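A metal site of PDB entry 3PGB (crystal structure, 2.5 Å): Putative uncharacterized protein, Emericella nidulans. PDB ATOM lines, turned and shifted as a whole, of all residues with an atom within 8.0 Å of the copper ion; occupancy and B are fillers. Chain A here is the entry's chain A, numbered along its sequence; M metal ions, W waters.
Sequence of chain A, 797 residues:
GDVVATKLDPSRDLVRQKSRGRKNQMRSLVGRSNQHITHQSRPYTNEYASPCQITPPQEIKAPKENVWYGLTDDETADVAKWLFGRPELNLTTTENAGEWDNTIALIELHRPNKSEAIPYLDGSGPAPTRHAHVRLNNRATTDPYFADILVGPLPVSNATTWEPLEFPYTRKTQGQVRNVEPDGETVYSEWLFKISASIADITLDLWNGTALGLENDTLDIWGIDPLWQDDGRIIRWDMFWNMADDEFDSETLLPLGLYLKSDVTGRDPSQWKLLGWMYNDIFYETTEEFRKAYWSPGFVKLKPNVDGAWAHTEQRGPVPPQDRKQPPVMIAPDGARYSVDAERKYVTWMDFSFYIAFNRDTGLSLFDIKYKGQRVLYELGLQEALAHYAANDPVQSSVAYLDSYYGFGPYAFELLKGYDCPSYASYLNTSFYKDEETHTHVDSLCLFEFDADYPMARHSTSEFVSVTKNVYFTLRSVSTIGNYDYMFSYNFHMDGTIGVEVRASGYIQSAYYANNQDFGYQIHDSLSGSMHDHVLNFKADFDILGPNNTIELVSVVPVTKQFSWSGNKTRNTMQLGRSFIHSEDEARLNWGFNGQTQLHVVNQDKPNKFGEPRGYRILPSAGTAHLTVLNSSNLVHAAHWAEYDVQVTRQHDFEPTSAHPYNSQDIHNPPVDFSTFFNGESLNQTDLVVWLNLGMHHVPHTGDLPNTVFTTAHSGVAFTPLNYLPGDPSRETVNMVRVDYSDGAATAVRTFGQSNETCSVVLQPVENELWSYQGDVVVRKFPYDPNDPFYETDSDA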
ATOM      1  N   ALA A 387      -3.290 -37.828  29.172  1.00  0.00           N
ATOM      2  CA  ALA A 387      -2.458 -36.699  28.793  1.00  0.00           C
ATOM      3  C   ALA A 387      -1.064 -37.230  28.465  1.00  0.00           C
ATOM      4  O   ALA A 387      -0.201 -37.344  29.337  1.00  0.00           O
ATOM      5  CB  ALA A 387      -2.385 -35.686  29.911  1.00  0.00           C
ATOM      6  N   TYR A 389       2.455 -36.951  26.752  1.00  0.00           N
ATOM      7  CA  TYR A 389       3.425 -35.942  26.322  1.00  0.00           C
ATOM      8  C   TYR A 389       4.564 -36.538  25.492  1.00  0.00           C
ATOM      9  O   TYR A 389       4.680 -37.749  25.332  1.00  0.00           O
ATOM     10  CB  TYR A 389       4.002 -35.215  27.534  1.00  0.00           C
ATOM     11  CG  TYR A 389       2.993 -34.332  28.224  1.00  0.00           C
ATOM     12  CD1 TYR A 389       2.005 -34.876  29.031  1.00  0.00           C
ATOM     13  CD2 TYR A 389       3.040 -32.956  28.072  1.00  0.00           C
ATOM     14  CE1 TYR A 389       1.080 -34.070  29.656  1.00  0.00           C
ATOM     15  CE2 TYR A 389       2.124 -32.149  28.687  1.00  0.00           C
ATOM     16  CZ  TYR A 389       1.148 -32.706  29.483  1.00  0.00           C
ATOM     17  OH  TYR A 389       0.238 -31.877  30.096  1.00  0.00           O
ATOM     18  N   ASN A 483      -3.173 -28.875  37.456  1.00  0.00           N
ATOM     19  CA  ASN A 483      -3.101 -27.756  36.515  1.00  0.00           C
ATOM     20  C   ASN A 483      -4.185 -27.743  35.426  1.00  0.00           C
ATOM     21  O   ASN A 483      -4.439 -26.702  34.827  1.00  0.00           O
ATOM     22  CB  ASN A 483      -1.720 -27.691  35.867  1.00  0.00           C
ATOM     23  CG  ASN A 483      -1.352 -28.988  35.150  1.00  0.00           C
ATOM     24  OD1 ASN A 483      -1.406 -30.061  35.736  1.00  0.00           O
ATOM     25  ND2 ASN A 483      -0.965 -28.867  33.884  1.00  0.00           N
ATOM     26  N   TPQ A 484      -4.827 -28.887  35.175  1.00  0.00           N
ATOM     27  CA  TPQ A 484      -5.842 -28.990  34.109  1.00  0.00           C
ATOM     28  CB  TPQ A 484      -6.011 -30.421  33.566  1.00  0.00           C
ATOM     29  C   TPQ A 484      -7.210 -28.584  34.615  1.00  0.00           C
ATOM     30  O   TPQ A 484      -7.583 -28.942  35.715  1.00  0.00           O
ATOM     31  C1  TPQ A 484      -4.682 -31.077  33.268  1.00  0.00           C
ATOM     32  C2  TPQ A 484      -3.950 -30.719  32.030  1.00  0.00           C
ATOM     33  O2  TPQ A 484      -4.437 -29.875  31.243  1.00  0.00           O
ATOM     34  C3  TPQ A 484      -2.649 -31.363  31.744  1.00  0.00           C
ATOM     35  C4  TPQ A 484      -2.122 -32.308  32.620  1.00  0.00           C
ATOM     36  O4  TPQ A 484      -1.021 -32.828  32.334  1.00  0.00           O
ATOM     37  C5  TPQ A 484      -2.857 -32.683  33.874  1.00  0.00           C
ATOM     38  O5  TPQ A 484      -2.413 -33.545  34.696  1.00  0.00           O
ATOM     39  C6  TPQ A 484      -4.160 -32.030  34.148  1.00  0.00           C
ATOM     40  N   TYR A 486     -10.813 -29.365  33.157  1.00  0.00           N
ATOM     41  CA  TYR A 486     -11.682 -30.002  32.193  1.00  0.00           C
ATOM     42  C   TYR A 486     -13.110 -29.610  32.486  1.00  0.00           C
ATOM     43  O   TYR A 486     -13.584 -29.829  33.594  1.00  0.00           O
ATOM     44  CB  TYR A 486     -11.546 -31.516  32.268  1.00  0.00           C
ATOM     45  CG  TYR A 486     -10.198 -32.043  31.834  1.00  0.00           C
ATOM     46  CD1 TYR A 486      -9.827 -32.029  30.491  1.00  0.00           C
ATOM     47  CD2 TYR A 486      -9.301 -32.561  32.760  1.00  0.00           C
ATOM     48  CE1 TYR A 486      -8.582 -32.525  30.082  1.00  0.00           C
ATOM     49  CE2 TYR A 486      -8.060 -33.059  32.367  1.00  0.00           C
ATOM     50  CZ  TYR A 486      -7.701 -33.037  31.023  1.00  0.00           C
ATOM     51  OH  TYR A 486      -6.477 -33.522  30.634  1.00  0.00           O
ATOM     52  N   ALA A 504     -10.958 -27.630  27.485  1.00  0.00           N
ATOM     53  CA  ALA A 504      -9.813 -27.571  28.381  1.00  0.00           C
ATOM     54  C   ALA A 504      -9.358 -26.127  28.584  1.00  0.00           C
ATOM     55  O   ALA A 504      -9.414 -25.312  27.673  1.00  0.00           O
ATOM     56  CB  ALA A 504      -8.664 -28.397  27.840  1.00  0.00           C
ATOM     57  N   SER A 505      -8.931 -25.830  29.806  1.00  0.00           N
ATOM     58  CA  SER A 505      -8.283 -24.582  30.142  1.00  0.00           C
ATOM     59  C   SER A 505      -7.304 -24.857  31.271  1.00  0.00           C
ATOM     60  O   SER A 505      -6.901 -26.000  31.454  1.00  0.00           O
ATOM     61  CB  SER A 505      -9.317 -23.534  30.552  1.00  0.00           C
ATOM     62  OG  SER A 505      -8.711 -22.259  30.701  1.00  0.00           O
ATOM     63  N   GLY A 506      -6.925 -23.835  32.018  1.00  0.00           N
ATOM     64  CA  GLY A 506      -5.954 -23.983  33.100  1.00  0.00           C
ATOM     65  C   GLY A 506      -4.525 -23.882  32.587  1.00  0.00           C
ATOM     66  O   GLY A 506      -4.283 -23.391  31.493  1.00  0.00           O
ATOM     67  N   TYR A 507      -3.593 -24.359  33.407  1.00  0.00           N
ATOM     68  CA  TYR A 507      -2.162 -24.240  33.118  1.00  0.00           C
ATOM     69  C   TYR A 507      -1.665 -25.427  32.326  1.00  0.00           C
ATOM     70  O   TYR A 507      -2.024 -26.573  32.612  1.00  0.00           O
ATOM     71  CB  TYR A 507      -1.363 -24.137  34.412  1.00  0.00           C
ATOM     72  CG  TYR A 507      -1.385 -22.757  35.009  1.00  0.00           C
ATOM     73  CD1 TYR A 507      -2.312 -22.407  35.978  1.00  0.00           C
ATOM     74  CD2 TYR A 507      -0.468 -21.797  34.620  1.00  0.00           C
ATOM     75  CE1 TYR A 507      -2.335 -21.143  36.526  1.00  0.00           C
ATOM     76  CE2 TYR A 507      -0.474 -20.532  35.166  1.00  0.00           C
ATOM     77  CZ  TYR A 507      -1.419 -20.217  36.121  1.00  0.00           C
ATOM     78  OH  TYR A 507      -1.447 -18.960  36.673  1.00  0.00           O
ATOM     79  N   ILE A 508      -0.826 -25.172  31.343  1.00  0.00           N
ATOM     80  CA  ILE A 508      -0.180 -26.243  30.619  1.00  0.00           C
ATOM     81  C   ILE A 508       0.950 -26.793  31.486  1.00  0.00           C
ATOM     82  O   ILE A 508       1.493 -26.092  32.339  1.00  0.00           O
ATOM     83  CB  ILE A 508       0.348 -25.780  29.234  1.00  0.00           C
ATOM     84  CG1 ILE A 508       1.535 -24.812  29.356  1.00  0.00           C
ATOM     85  CG2 ILE A 508      -0.778 -25.151  28.425  1.00  0.00           C
ATOM     86  CD1 ILE A 508       2.174 -24.444  28.012  1.00  0.00           C
ATOM     87  N   GLN A 509       1.302 -28.067  31.288  1.00  0.00           N
ATOM     88  CA  GLN A 509       2.504 -28.593  31.882  1.00  0.00           C
ATOM     89  C   GLN A 509       3.634 -28.341  30.899  1.00  0.00           C
ATOM     90  O   GLN A 509       3.726 -28.974  29.846  1.00  0.00           O
ATOM     91  CB  GLN A 509       2.403 -30.075  32.219  1.00  0.00           C
ATOM     92  CG  GLN A 509       3.575 -30.516  33.073  1.00  0.00           C
ATOM     93  CD  GLN A 509       3.424 -31.917  33.579  1.00  0.00           C
ATOM     94  OE1 GLN A 509       4.079 -32.833  33.072  1.00  0.00           O
ATOM     95  NE2 GLN A 509       2.571 -32.108  34.566  1.00  0.00           N
ATOM     96  N   GLY A 529       6.410 -24.642  25.024  1.00  0.00           N
ATOM     97  CA  GLY A 529       5.020 -24.997  25.189  1.00  0.00           C
ATOM     98  C   GLY A 529       4.837 -26.496  25.276  1.00  0.00           C
ATOM     99  O   GLY A 529       3.868 -26.960  25.875  1.00  0.00           O
ATOM    100  N   MET A 531       4.333 -30.515  23.937  1.00  0.00           N
ATOM    101  CA  MET A 531       3.270 -31.103  23.146  1.00  0.00           C
ATOM    102  C   MET A 531       2.624 -32.254  23.893  1.00  0.00           C
ATOM    103  O   MET A 531       3.295 -32.935  24.654  1.00  0.00           O
ATOM    104  CB  MET A 531       3.792 -31.582  21.787  1.00  0.00           C
ATOM    105  CG  MET A 531       4.888 -32.635  21.841  1.00  0.00           C
ATOM    106  SD  MET A 531       5.557 -33.033  20.216  1.00  0.00           S
ATOM    107  CE  MET A 531       4.098 -33.682  19.391  1.00  0.00           C
ATOM    108  N   HIS A 532       1.327 -32.453  23.685  1.00  0.00           N
ATOM    109  CA  HIS A 532       0.633 -33.569  24.304  1.00  0.00           C
ATOM    110  C   HIS A 532      -0.689 -33.866  23.606  1.00  0.00           C
ATOM    111  O   HIS A 532      -1.299 -32.979  22.996  1.00  0.00           O
ATOM    112  CB  HIS A 532       0.391 -33.307  25.798  1.00  0.00           C
ATOM    113  CG  HIS A 532      -0.354 -32.034  26.083  1.00  0.00           C
ATOM    114  ND1 HIS A 532       0.296 -30.824  26.242  1.00  0.00           N
ATOM    115  CD2 HIS A 532      -1.676 -31.780  26.219  1.00  0.00           C
ATOM    116  CE1 HIS A 532      -0.609 -29.881  26.463  1.00  0.00           C
ATOM    117  NE2 HIS A 532      -1.812 -30.435  26.460  1.00  0.00           N
ATOM    118  N   ASP A 533      -1.112 -35.126  23.683  1.00  0.00           N
ATOM    119  CA  ASP A 533      -2.433 -35.533  23.213  1.00  0.00           C
ATOM    120  C   ASP A 533      -3.383 -35.670  24.409  1.00  0.00           C
ATOM    121  O   ASP A 533      -3.062 -36.339  25.396  1.00  0.00           O
ATOM    122  CB  ASP A 533      -2.376 -36.859  22.458  1.00  0.00           C
ATOM    123  CG  ASP A 533      -1.950 -36.703  21.001  1.00  0.00           C
ATOM    124  OD1 ASP A 533      -1.688 -35.568  20.534  1.00  0.00           O
ATOM    125  OD2 ASP A 533      -1.881 -37.753  20.315  1.00  0.00           O
ATOM    126  N   HIS A 534      -4.530 -35.011  24.310  1.00  0.00           N
ATOM    127  CA  HIS A 534      -5.626 -35.255  25.225  1.00  0.00           C
ATOM    128  C   HIS A 534      -6.483 -36.324  24.569  1.00  0.00           C
ATOM    129  O   HIS A 534      -6.904 -36.166  23.423  1.00  0.00           O
ATOM    130  CB  HIS A 534      -6.483 -34.018  25.418  1.00  0.00           C
ATOM    131  CG  HIS A 534      -5.820 -32.921  26.178  1.00  0.00           C
ATOM    132  ND1 HIS A 534      -5.749 -32.896  27.551  1.00  0.00           N
ATOM    133  CD2 HIS A 534      -5.225 -31.784  25.753  1.00  0.00           C
ATOM    134  CE1 HIS A 534      -5.127 -31.802  27.936  1.00  0.00           C
ATOM    135  NE2 HIS A 534      -4.801 -31.106  26.867  1.00  0.00           N
ATOM    136  N   MET A 696      -7.701 -34.115  21.609  1.00  0.00           N
ATOM    137  CA  MET A 696      -7.057 -32.981  20.956  1.00  0.00           C
ATOM    138  C   MET A 696      -5.560 -33.220  20.830  1.00  0.00           C
ATOM    139  O   MET A 696      -4.959 -33.810  21.728  1.00  0.00           O
ATOM    140  CB  MET A 696      -7.215 -31.715  21.793  1.00  0.00           C
ATOM    141  CG  MET A 696      -8.614 -31.193  21.940  1.00  0.00           C
ATOM    142  SD  MET A 696      -8.910 -30.625  23.629  1.00  0.00           S
ATOM    143  CE  MET A 696      -9.732 -32.058  24.329  1.00  0.00           C
ATOM    144  N   HIS A 697      -4.962 -32.731  19.746  1.00  0.00           N
ATOM    145  CA  HIS A 697      -3.512 -32.632  19.652  1.00  0.00           C
ATOM    146  C   HIS A 697      -3.169 -31.212  20.069  1.00  0.00           C
ATOM    147  O   HIS A 697      -3.577 -30.253  19.410  1.00  0.00           O
ATOM    148  CB  HIS A 697      -3.019 -32.898  18.231  1.00  0.00           C
ATOM    149  CG  HIS A 697      -3.442 -34.218  17.668  1.00  0.00           C
ATOM    150  ND1 HIS A 697      -2.931 -35.417  18.123  1.00  0.00           N
ATOM    151  CD2 HIS A 697      -4.321 -34.527  16.690  1.00  0.00           C
ATOM    152  CE1 HIS A 697      -3.479 -36.407  17.445  1.00  0.00           C
ATOM    153  NE2 HIS A 697      -4.325 -35.886  16.568  1.00  0.00           N
ATOM    154  N   HIS A 698      -2.430 -31.075  21.166  1.00  0.00           N
ATOM    155  CA  HIS A 698      -2.167 -29.767  21.748  1.00  0.00           C
ATOM    156  C   HIS A 698      -0.676 -29.480  21.769  1.00  0.00           C
ATOM    157  O   HIS A 698       0.075 -30.063  22.549  1.00  0.00           O
ATOM    158  CB  HIS A 698      -2.767 -29.700  23.150  1.00  0.00           C
ATOM    159  CG  HIS A 698      -2.837 -28.325  23.722  1.00  0.00           C
ATOM    160  ND1 HIS A 698      -3.118 -28.081  25.050  1.00  0.00           N
ATOM    161  CD2 HIS A 698      -2.652 -27.109  23.156  1.00  0.00           C
ATOM    162  CE1 HIS A 698      -3.116 -26.775  25.274  1.00  0.00           C
ATOM    163  NE2 HIS A 698      -2.828 -26.165  24.138  1.00  0.00           N
ATOM    164  N   VAL A 699      -0.258 -28.574  20.878  1.00  0.00           N
ATOM    165  CA  VAL A 699       1.084 -28.031  20.866  1.00  0.00           C
ATOM    166  C   VAL A 699       0.989 -26.580  21.321  1.00  0.00           C
ATOM    167  O   VAL A 699       0.840 -25.684  20.498  1.00  0.00           O
ATOM    168  CB  VAL A 699       1.718 -28.111  19.460  1.00  0.00           C
ATOM    169  CG1 VAL A 699       3.172 -27.657  19.501  1.00  0.00           C
ATOM    170  CG2 VAL A 699       1.618 -29.527  18.912  1.00  0.00           C
ATOM    171  N   PRO A 700       1.073 -26.337  22.650  1.00  0.00           N
ATOM    172  CA  PRO A 700       0.812 -24.995  23.159  1.00  0.00           C
ATOM    173  C   PRO A 700       1.714 -23.921  22.582  1.00  0.00           C
ATOM    174  O   PRO A 700       2.940 -24.117  22.482  1.00  0.00           O
ATOM    175  CB  PRO A 700       1.081 -25.158  24.662  1.00  0.00           C
ATOM    176  CG  PRO A 700       0.855 -26.563  24.928  1.00  0.00           C
ATOM    177  CD  PRO A 700       1.411 -27.252  23.746  1.00  0.00           C
ATOM    178  N   ASP A 704      -1.289 -19.755  24.906  1.00  0.00           N
ATOM    179  CA  ASP A 704      -1.592 -20.615  26.045  1.00  0.00           C
ATOM    180  C   ASP A 704      -1.025 -20.041  27.357  1.00  0.00           C
ATOM    181  O   ASP A 704      -1.182 -20.654  28.405  1.00  0.00           O
ATOM    182  CB  ASP A 704      -1.091 -22.036  25.785  1.00  0.00           C
ATOM    183  CG  ASP A 704      -1.888 -22.731  24.701  1.00  0.00           C
ATOM    184  OD1 ASP A 704      -2.954 -23.284  25.044  1.00  0.00           O
ATOM    185  OD2 ASP A 704      -1.472 -22.726  23.530  1.00  0.00           O
ATOM    186  N   THR A 708      -4.509 -21.946  28.916  1.00  0.00           N
ATOM    187  CA  THR A 708      -5.163 -22.397  27.704  1.00  0.00           C
ATOM    188  C   THR A 708      -6.610 -21.901  27.757  1.00  0.00           C
ATOM    189  O   THR A 708      -7.156 -21.714  28.845  1.00  0.00           O
ATOM    190  CB  THR A 708      -5.109 -23.927  27.583  1.00  0.00           C
ATOM    191  OG1 THR A 708      -3.740 -24.331  27.526  1.00  0.00           O
ATOM    192  CG2 THR A 708      -5.829 -24.431  26.330  1.00  0.00           C
ATOM    193  N   ALA A 713      -9.608 -25.144  22.681  1.00  0.00           N
ATOM    194  CA  ALA A 713      -9.358 -26.457  23.286  1.00  0.00           C
ATOM    195  C   ALA A 713     -10.704 -27.151  23.514  1.00  0.00           C
ATOM    196  O   ALA A 713     -11.269 -27.121  24.603  1.00  0.00           O
ATOM    197  CB  ALA A 713      -8.589 -26.319  24.582  1.00  0.00           C
HETATM  198 CU    CU M   1      -3.593 -29.461  26.436  1.00  0.00          CU
HETATM  199  O   HOH W   1      -3.440 -28.305  28.625  1.00  0.00           O
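A ring nitrogen (ND1) of His 534 is in hydrogen-bond range of the side-chain hydroxyl (OH) of Tyr 486. The side-chain carboxylate (OD1) of Asp 704 lies within hydrogen-bond range of a ring nitrogen (NE2) of His 698 (3.0 Å). The backbone carbonyl oxygen (O) of His 534 lies within hydrogen-bond range of the backbone NH (N) of Met 696, at 2.9 Å.
Within 4 Å of the copper ion: His 532, His 534 and His 698.
The copper ion is bound by a ring nitrogen (ND1) of His 698 (2.0 Å), a ring nitrogen (NE2) of His 532 (2.0 Å), a ring nitrogen (NE2) of His 534 (2.1 Å) and water W1 (2.5 Å). The copper ion has four donor atoms within binding distance.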
